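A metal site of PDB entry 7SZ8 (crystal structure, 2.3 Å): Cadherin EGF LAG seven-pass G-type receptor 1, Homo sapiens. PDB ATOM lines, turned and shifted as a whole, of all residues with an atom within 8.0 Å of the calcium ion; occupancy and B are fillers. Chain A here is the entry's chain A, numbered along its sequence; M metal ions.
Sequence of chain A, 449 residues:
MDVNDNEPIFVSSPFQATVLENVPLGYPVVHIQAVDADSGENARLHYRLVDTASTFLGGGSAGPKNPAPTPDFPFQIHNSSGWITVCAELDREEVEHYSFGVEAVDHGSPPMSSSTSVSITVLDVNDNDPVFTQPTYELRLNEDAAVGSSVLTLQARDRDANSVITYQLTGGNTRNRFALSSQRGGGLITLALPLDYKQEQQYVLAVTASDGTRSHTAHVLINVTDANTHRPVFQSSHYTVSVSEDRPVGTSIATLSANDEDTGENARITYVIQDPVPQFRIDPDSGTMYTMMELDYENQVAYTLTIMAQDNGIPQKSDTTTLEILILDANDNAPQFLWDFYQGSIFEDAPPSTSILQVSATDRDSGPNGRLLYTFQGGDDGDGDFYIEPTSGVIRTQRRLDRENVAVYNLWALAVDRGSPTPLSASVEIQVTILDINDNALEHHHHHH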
ATOM      1  N   ASP A 226     -24.188 -24.109  -9.950  1.00  0.00           N
ATOM      2  CA  ASP A 226     -24.685 -23.222 -11.026  1.00  0.00           C
ATOM      3  C   ASP A 226     -26.212 -23.092 -10.915  1.00  0.00           C
ATOM      4  O   ASP A 226     -26.818 -24.165 -10.680  1.00  0.00           O
ATOM      5  CB  ASP A 226     -24.370 -23.727 -12.427  1.00  0.00           C
ATOM      6  CG  ASP A 226     -24.682 -22.688 -13.498  1.00  0.00           C
ATOM      7  OD1 ASP A 226     -24.409 -21.444 -13.285  1.00  0.00           O
ATOM      8  OD2 ASP A 226     -25.157 -23.114 -14.546  1.00  0.00           O
ATOM      9  N   ALA A 227     -26.741 -21.863 -11.024  1.00  0.00           N
ATOM     10  CA  ALA A 227     -28.169 -21.500 -11.163  1.00  0.00           C
ATOM     11  C   ALA A 227     -28.399 -20.742 -12.485  1.00  0.00           C
ATOM     12  O   ALA A 227     -27.418 -20.221 -13.072  1.00  0.00           O
ATOM     13  CB  ALA A 227     -28.604 -20.659  -9.996  1.00  0.00           C
ATOM     14  N   ASN A 228     -29.659 -20.637 -12.924  1.00  0.00           N
ATOM     15  CA  ASN A 228     -30.064 -19.931 -14.173  1.00  0.00           C
ATOM     16  C   ASN A 228     -30.202 -18.434 -13.892  1.00  0.00           C
ATOM     17  O   ASN A 228     -31.342 -17.944 -13.832  1.00  0.00           O
ATOM     18  CB  ASN A 228     -31.341 -20.506 -14.792  1.00  0.00           C
ATOM     19  CG  ASN A 228     -31.413 -20.190 -16.282  1.00  0.00           C
ATOM     20  OD1 ASN A 228     -30.383 -20.061 -16.944  1.00  0.00           O
ATOM     21  ND2 ASN A 228     -32.626 -20.102 -16.821  1.00  0.00           N
ATOM     22  N   THR A 229     -29.073 -17.734 -13.708  1.00  0.00           N
ATOM     23  CA  THR A 229     -29.032 -16.289 -13.329  1.00  0.00           C
ATOM     24  C   THR A 229     -28.916 -15.406 -14.576  1.00  0.00           C
ATOM     25  O   THR A 229     -28.946 -14.201 -14.410  1.00  0.00           O
ATOM     26  CB  THR A 229     -27.910 -16.005 -12.327  1.00  0.00           C
ATOM     27  OG1 THR A 229     -26.712 -16.540 -12.867  1.00  0.00           O
ATOM     28  CG2 THR A 229     -28.191 -16.636 -10.976  1.00  0.00           C
ATOM     29  N   HIS A 230     -28.879 -15.978 -15.780  1.00  0.00           N
ATOM     30  CA  HIS A 230     -28.758 -15.213 -17.050  1.00  0.00           C
ATOM     31  C   HIS A 230     -29.781 -15.652 -18.105  1.00  0.00           C
ATOM     32  O   HIS A 230     -30.177 -16.839 -18.111  1.00  0.00           O
ATOM     33  CB  HIS A 230     -27.349 -15.323 -17.640  1.00  0.00           C
ATOM     34  CG  HIS A 230     -26.264 -14.948 -16.701  1.00  0.00           C
ATOM     35  ND1 HIS A 230     -25.849 -15.794 -15.695  1.00  0.00           N
ATOM     36  CD2 HIS A 230     -25.520 -13.824 -16.589  1.00  0.00           C
ATOM     37  CE1 HIS A 230     -24.872 -15.204 -15.018  1.00  0.00           C
ATOM     38  NE2 HIS A 230     -24.643 -13.997 -15.555  1.00  0.00           N
ATOM     39  N   ARG A 231     -30.147 -14.686 -18.937  1.00  0.00           N
ATOM     40  CA  ARG A 231     -31.025 -14.797 -20.129  1.00  0.00           C
ATOM     41  C   ARG A 231     -30.058 -14.928 -21.306  1.00  0.00           C
ATOM     42  O   ARG A 231     -28.991 -14.333 -21.286  1.00  0.00           O
ATOM     43  CB  ARG A 231     -31.962 -13.584 -20.177  1.00  0.00           C
ATOM     44  CG  ARG A 231     -32.701 -13.363 -18.850  1.00  0.00           C
ATOM     45  CD  ARG A 231     -33.661 -12.178 -18.668  1.00  0.00           C
ATOM     46  NE  ARG A 231     -34.336 -11.925 -19.918  1.00  0.00           N
ATOM     47  CZ  ARG A 231     -34.401 -10.756 -20.574  1.00  0.00           C
ATOM     48  NH1 ARG A 231     -33.938  -9.636 -20.040  1.00  0.00           N
ATOM     49  NH2 ARG A 231     -34.974 -10.721 -21.752  1.00  0.00           N
ATOM     50  N   PRO A 232     -30.339 -15.743 -22.326  1.00  0.00           N
ATOM     51  CA  PRO A 232     -29.640 -15.610 -23.604  1.00  0.00           C
ATOM     52  C   PRO A 232     -29.637 -14.138 -24.004  1.00  0.00           C
ATOM     53  O   PRO A 232     -30.592 -13.413 -23.629  1.00  0.00           O
ATOM     54  CB  PRO A 232     -30.498 -16.465 -24.540  1.00  0.00           C
ATOM     55  CG  PRO A 232     -31.009 -17.554 -23.638  1.00  0.00           C
ATOM     56  CD  PRO A 232     -31.335 -16.826 -22.344  1.00  0.00           C
ATOM     57  N   ASN A 259     -25.814 -15.918 -26.911  1.00  0.00           N
ATOM     58  CA  ASN A 259     -24.832 -16.408 -25.920  1.00  0.00           C
ATOM     59  C   ASN A 259     -25.377 -16.210 -24.500  1.00  0.00           C
ATOM     60  O   ASN A 259     -25.919 -15.132 -24.157  1.00  0.00           O
ATOM     61  CB  ASN A 259     -23.478 -15.770 -26.193  1.00  0.00           C
ATOM     62  CG  ASN A 259     -22.413 -16.197 -25.216  1.00  0.00           C
ATOM     63  OD1 ASN A 259     -22.234 -17.389 -24.972  1.00  0.00           O
ATOM     64  ND2 ASN A 259     -21.744 -15.221 -24.615  1.00  0.00           N
ATOM     65  N   ASP A 260     -25.234 -17.264 -23.679  1.00  0.00           N
ATOM     66  CA  ASP A 260     -25.732 -17.354 -22.286  1.00  0.00           C
ATOM     67  C   ASP A 260     -24.522 -17.603 -21.380  1.00  0.00           C
ATOM     68  O   ASP A 260     -23.779 -18.573 -21.632  1.00  0.00           O
ATOM     69  CB  ASP A 260     -26.838 -18.407 -22.208  1.00  0.00           C
ATOM     70  CG  ASP A 260     -27.718 -18.370 -20.969  1.00  0.00           C
ATOM     71  OD1 ASP A 260     -27.171 -18.389 -19.863  1.00  0.00           O
ATOM     72  OD2 ASP A 260     -28.976 -18.319 -21.152  1.00  0.00           O
ATOM     73  N   GLU A 261     -24.334 -16.726 -20.385  1.00  0.00           N
ATOM     74  CA  GLU A 261     -23.241 -16.745 -19.372  1.00  0.00           C
ATOM     75  C   GLU A 261     -23.406 -17.859 -18.330  1.00  0.00           C
ATOM     76  O   GLU A 261     -22.480 -17.994 -17.512  1.00  0.00           O
ATOM     77  CB  GLU A 261     -23.219 -15.412 -18.595  1.00  0.00           C
ATOM     78  CG  GLU A 261     -22.890 -14.176 -19.413  1.00  0.00           C
ATOM     79  CD  GLU A 261     -22.555 -12.992 -18.513  1.00  0.00           C
ATOM     80  OE1 GLU A 261     -23.270 -11.920 -18.561  1.00  0.00           O
ATOM     81  OE2 GLU A 261     -21.609 -13.128 -17.737  1.00  0.00           O
ATOM     82  N   ASP A 262     -24.525 -18.605 -18.268  1.00  0.00           N
ATOM     83  CA  ASP A 262     -24.703 -19.726 -17.306  1.00  0.00           C
ATOM     84  C   ASP A 262     -23.912 -20.954 -17.813  1.00  0.00           C
ATOM     85  O   ASP A 262     -23.123 -20.770 -18.756  1.00  0.00           O
ATOM     86  CB  ASP A 262     -26.196 -20.009 -17.099  1.00  0.00           C
ATOM     87  CG  ASP A 262     -26.936 -18.876 -16.410  1.00  0.00           C
ATOM     88  OD1 ASP A 262     -26.399 -18.365 -15.376  1.00  0.00           O
ATOM     89  OD2 ASP A 262     -28.010 -18.482 -16.920  1.00  0.00           O
ATOM     90  N   THR A 263     -24.111 -22.150 -17.223  1.00  0.00           N
ATOM     91  CA  THR A 263     -23.421 -23.416 -17.615  1.00  0.00           C
ATOM     92  C   THR A 263     -24.472 -24.486 -17.993  1.00  0.00           C
ATOM     93  O   THR A 263     -25.616 -24.438 -17.490  1.00  0.00           O
ATOM     94  CB  THR A 263     -22.492 -23.944 -16.496  1.00  0.00           C
ATOM     95  OG1 THR A 263     -21.555 -22.941 -16.092  1.00  0.00           O
ATOM     96  CG2 THR A 263     -21.709 -25.186 -16.890  1.00  0.00           C
ATOM     97  N   GLY A 264     -24.075 -25.434 -18.839  1.00  0.00           N
ATOM     98  CA  GLY A 264     -24.855 -26.644 -19.153  1.00  0.00           C
ATOM     99  C   GLY A 264     -26.143 -26.288 -19.846  1.00  0.00           C
ATOM    100  O   GLY A 264     -26.087 -25.488 -20.809  1.00  0.00           O
ATOM    101  N   GLU A 265     -27.250 -26.863 -19.356  1.00  0.00           N
ATOM    102  CA  GLU A 265     -28.640 -26.669 -19.808  1.00  0.00           C
ATOM    103  C   GLU A 265     -29.055 -25.220 -19.555  1.00  0.00           C
ATOM    104  O   GLU A 265     -29.755 -24.617 -20.416  1.00  0.00           O
ATOM    105  CB  GLU A 265     -29.581 -27.609 -19.064  1.00  0.00           C
ATOM    106  CG  GLU A 265     -29.336 -29.075 -19.399  1.00  0.00           C
ATOM    107  CD  GLU A 265     -29.791 -29.434 -20.812  1.00  0.00           C
ATOM    108  OE1 GLU A 265     -31.024 -29.491 -21.011  1.00  0.00           O
ATOM    109  OE2 GLU A 265     -28.921 -29.578 -21.726  1.00  0.00           O
ATOM    110  N   ASN A 266     -28.641 -24.658 -18.429  1.00  0.00           N
ATOM    111  CA  ASN A 266     -28.878 -23.216 -18.110  1.00  0.00           C
ATOM    112  C   ASN A 266     -28.402 -22.271 -19.244  1.00  0.00           C
ATOM    113  O   ASN A 266     -28.941 -21.146 -19.314  1.00  0.00           O
ATOM    114  CB  ASN A 266     -28.266 -22.877 -16.769  1.00  0.00           C
ATOM    115  CG  ASN A 266     -28.850 -23.713 -15.644  1.00  0.00           C
ATOM    116  OD1 ASN A 266     -29.964 -24.212 -15.759  1.00  0.00           O
ATOM    117  ND2 ASN A 266     -28.083 -23.870 -14.576  1.00  0.00           N
ATOM    118  N   ALA A 267     -27.479 -22.721 -20.122  1.00  0.00           N
ATOM    119  CA  ALA A 267     -26.810 -21.955 -21.213  1.00  0.00           C
ATOM    120  C   ALA A 267     -27.085 -22.538 -22.603  1.00  0.00           C
ATOM    121  O   ALA A 267     -26.673 -21.876 -23.559  1.00  0.00           O
ATOM    122  CB  ALA A 267     -25.304 -21.954 -20.992  1.00  0.00           C
ATOM    123  N   ARG A 268     -27.618 -23.752 -22.727  1.00  0.00           N
ATOM    124  CA  ARG A 268     -27.953 -24.353 -24.039  1.00  0.00           C
ATOM    125  C   ARG A 268     -29.221 -23.694 -24.620  1.00  0.00           C
ATOM    126  O   ARG A 268     -30.282 -23.703 -23.940  1.00  0.00           O
ATOM    127  CB  ARG A 268     -28.164 -25.867 -23.931  1.00  0.00           C
ATOM    128  CG  ARG A 268     -28.560 -26.547 -25.245  1.00  0.00           C
ATOM    129  CD  ARG A 268     -28.593 -28.063 -25.137  1.00  0.00           C
ATOM    130  NE  ARG A 268     -29.715 -28.529 -24.317  1.00  0.00           N
ATOM    131  CZ  ARG A 268     -31.024 -28.528 -24.684  1.00  0.00           C
ATOM    132  NH1 ARG A 268     -31.385 -28.134 -25.889  1.00  0.00           N
ATOM    133  NH2 ARG A 268     -31.948 -28.983 -23.844  1.00  0.00           N
ATOM    134  N   ILE A 269     -29.103 -23.209 -25.852  1.00  0.00           N
ATOM    135  CA  ILE A 269     -30.115 -22.352 -26.518  1.00  0.00           C
ATOM    136  C   ILE A 269     -30.980 -23.236 -27.404  1.00  0.00           C
ATOM    137  O   ILE A 269     -30.435 -24.014 -28.178  1.00  0.00           O
ATOM    138  CB  ILE A 269     -29.426 -21.251 -27.358  1.00  0.00           C
ATOM    139  CG1 ILE A 269     -28.452 -20.426 -26.511  1.00  0.00           C
ATOM    140  CG2 ILE A 269     -30.435 -20.368 -28.044  1.00  0.00           C
ATOM    141  CD1 ILE A 269     -29.122 -19.676 -25.371  1.00  0.00           C
ATOM    142  N   GLN A 310     -34.380 -19.520 -26.163  1.00  0.00           N
ATOM    143  CA  GLN A 310     -34.670 -19.871 -24.763  1.00  0.00           C
ATOM    144  C   GLN A 310     -33.534 -20.753 -24.297  1.00  0.00           C
ATOM    145  O   GLN A 310     -33.120 -21.616 -25.080  1.00  0.00           O
ATOM    146  CB  GLN A 310     -36.022 -20.573 -24.585  1.00  0.00           C
ATOM    147  CG  GLN A 310     -36.366 -21.515 -25.727  1.00  0.00           C
ATOM    148  CD  GLN A 310     -37.593 -22.358 -25.456  1.00  0.00           C
ATOM    149  OE1 GLN A 310     -37.522 -23.568 -25.499  1.00  0.00           O
ATOM    150  NE2 GLN A 310     -38.735 -21.735 -25.224  1.00  0.00           N
ATOM    151  N   ASP A 311     -33.054 -20.524 -23.076  1.00  0.00           N
ATOM    152  CA  ASP A 311     -32.120 -21.476 -22.447  1.00  0.00           C
ATOM    153  C   ASP A 311     -32.959 -22.676 -21.988  1.00  0.00           C
ATOM    154  O   ASP A 311     -34.221 -22.641 -22.153  1.00  0.00           O
ATOM    155  CB  ASP A 311     -31.312 -20.850 -21.315  1.00  0.00           C
ATOM    156  CG  ASP A 311     -32.137 -20.397 -20.127  1.00  0.00           C
ATOM    157  OD1 ASP A 311     -33.231 -20.941 -19.899  1.00  0.00           O
ATOM    158  OD2 ASP A 311     -31.643 -19.527 -19.418  1.00  0.00           O
ATOM    159  N   ASN A 312     -32.289 -23.678 -21.435  1.00  0.00           N
ATOM    160  CA  ASN A 312     -32.933 -24.943 -21.018  1.00  0.00           C
ATOM    161  C   ASN A 312     -32.814 -25.069 -19.495  1.00  0.00           C
ATOM    162  O   ASN A 312     -32.932 -26.115 -18.985  1.00  0.00           O
ATOM    163  CB  ASN A 312     -32.402 -26.058 -21.918  1.00  0.00           C
ATOM    164  CG  ASN A 312     -33.170 -26.110 -23.221  1.00  0.00           C
ATOM    165  OD1 ASN A 312     -34.269 -26.652 -23.250  1.00  0.00           O
ATOM    166  ND2 ASN A 312     -32.628 -25.533 -24.281  1.00  0.00           N
ATOM    167  N   GLY A 313     -32.656 -23.951 -18.804  1.00  0.00           N
ATOM    168  CA  GLY A 313     -32.614 -23.910 -17.338  1.00  0.00           C
ATOM    169  C   GLY A 313     -34.007 -24.058 -16.742  1.00  0.00           C
ATOM    170  O   GLY A 313     -35.006 -24.010 -17.474  1.00  0.00           O
ATOM    171  N   ILE A 314     -34.051 -24.297 -15.445  1.00  0.00           N
ATOM    172  CA  ILE A 314     -35.284 -24.439 -14.642  1.00  0.00           C
ATOM    173  C   ILE A 314     -35.204 -23.370 -13.567  1.00  0.00           C
ATOM    174  O   ILE A 314     -34.207 -23.275 -12.885  1.00  0.00           O
ATOM    175  CB  ILE A 314     -35.372 -25.869 -14.049  1.00  0.00           C
ATOM    176  CG1 ILE A 314     -35.064 -26.951 -15.099  1.00  0.00           C
ATOM    177  CG2 ILE A 314     -36.721 -26.074 -13.376  1.00  0.00           C
ATOM    178  CD1 ILE A 314     -34.979 -28.367 -14.520  1.00  0.00           C
ATOM    179  N   PRO A 315     -36.119 -22.386 -13.528  1.00  0.00           N
ATOM    180  CA  PRO A 315     -36.979 -22.080 -14.651  1.00  0.00           C
ATOM    181  C   PRO A 315     -36.195 -21.427 -15.790  1.00  0.00           C
ATOM    182  O   PRO A 315     -35.183 -20.798 -15.550  1.00  0.00           O
ATOM    183  CB  PRO A 315     -37.897 -20.996 -14.095  1.00  0.00           C
ATOM    184  CG  PRO A 315     -37.015 -20.267 -13.118  1.00  0.00           C
ATOM    185  CD  PRO A 315     -36.266 -21.399 -12.438  1.00  0.00           C
ATOM    186  N   GLN A 316     -36.802 -21.478 -16.951  1.00  0.00           N
ATOM    187  CA  GLN A 316     -36.293 -21.082 -18.263  1.00  0.00           C
ATOM    188  C   GLN A 316     -36.280 -19.548 -18.436  1.00  0.00           C
ATOM    189  O   GLN A 316     -37.263 -18.860 -17.967  1.00  0.00           O
ATOM    190  CB  GLN A 316     -37.254 -21.760 -19.225  1.00  0.00           C
ATOM    191  CG  GLN A 316     -36.631 -22.143 -20.533  1.00  0.00           C
ATOM    192  CD  GLN A 316     -37.473 -23.184 -21.202  1.00  0.00           C
ATOM    193  OE1 GLN A 316     -38.566 -23.466 -20.774  1.00  0.00           O
ATOM    194  NE2 GLN A 316     -36.973 -23.731 -22.280  1.00  0.00           N
ATOM    195  N   LYS A 317     -35.254 -19.018 -19.100  1.00  0.00           N
ATOM    196  CA  LYS A 317     -35.200 -17.609 -19.531  1.00  0.00           C
ATOM    197  C   LYS A 317     -34.981 -17.546 -21.043  1.00  0.00           C
ATOM    198  O   LYS A 317     -34.522 -18.559 -21.617  1.00  0.00           O
ATOM    199  CB  LYS A 317     -34.097 -16.888 -18.783  1.00  0.00           C
ATOM    200  CG  LYS A 317     -34.410 -16.634 -17.314  1.00  0.00           C
ATOM    201  CD  LYS A 317     -33.150 -16.462 -16.481  1.00  0.00           C
ATOM    202  CE  LYS A 317     -33.269 -15.359 -15.459  1.00  0.00           C
ATOM    203  NZ  LYS A 317     -33.336 -15.932 -14.098  1.00  0.00           N
ATOM    204  N   SER A 318     -35.259 -16.392 -21.655  1.00  0.00           N
ATOM    205  CA  SER A 318     -35.335 -16.224 -23.117  1.00  0.00           C
ATOM    206  C   SER A 318     -35.030 -14.768 -23.486  1.00  0.00           C
ATOM    207  O   SER A 318     -35.146 -13.865 -22.613  1.00  0.00           O
ATOM    208  CB  SER A 318     -36.675 -16.602 -23.666  1.00  0.00           C
ATOM    209  OG  SER A 318     -37.638 -15.534 -23.500  1.00  0.00           O
HETATM  210 CA    CA M   1     -29.329 -19.059 -18.751  1.00  0.00          CA
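The calcium ion is bound by the backbone carbonyl oxygen (O) of Asn 266 (2.2 Å), the side-chain amide oxygen (OD1) of Asn 228 (2.3 Å), the side-chain carboxylate (OD2) of Asp 262 (2.3 Å), the side-chain carboxylate (OD2) of Asp 311 (2.5 Å), the backbone carbonyl oxygen (O) of His 230 (2.5 Å), the side-chain carboxylate (OD1) of Asp 260 (2.5 Å) and the side-chain carboxylate (OD2) of Asp 260 (2.5 Å).
The side-chain carboxylate of Asp 226 is in hydrogen-bond range of the side-chain amide nitrogen of Asn 266 (3.0 Å). O of Asn 228 sits at hydrogen-bond distance from NZ of Lys 317 (2.8 Å). ND2 of Asn 228 is in hydrogen-bond range of O of Pro 315 (2.9 Å). The side-chain hydroxyl of Thr 229 sits at hydrogen-bond distance from the side-chain carboxylate of Asp 262, at 3.1 Å. N of Asp 311 lies within hydrogen-bond range of O of Lys 317, at 2.9 Å. OD1 of Asp 311 sits at hydrogen-bond distance from N of Gly 313 (3.3 Å). The backbone carbonyl oxygen (O) of Asp 311 sits close to the side-chain amide nitrogen (NE2) of Gln 316. The side-chain hydroxyl (OG1) of Thr 229 sits at hydrogen-bond distance from a ring nitrogen (ND1) of His 230, at 3.0 Å.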
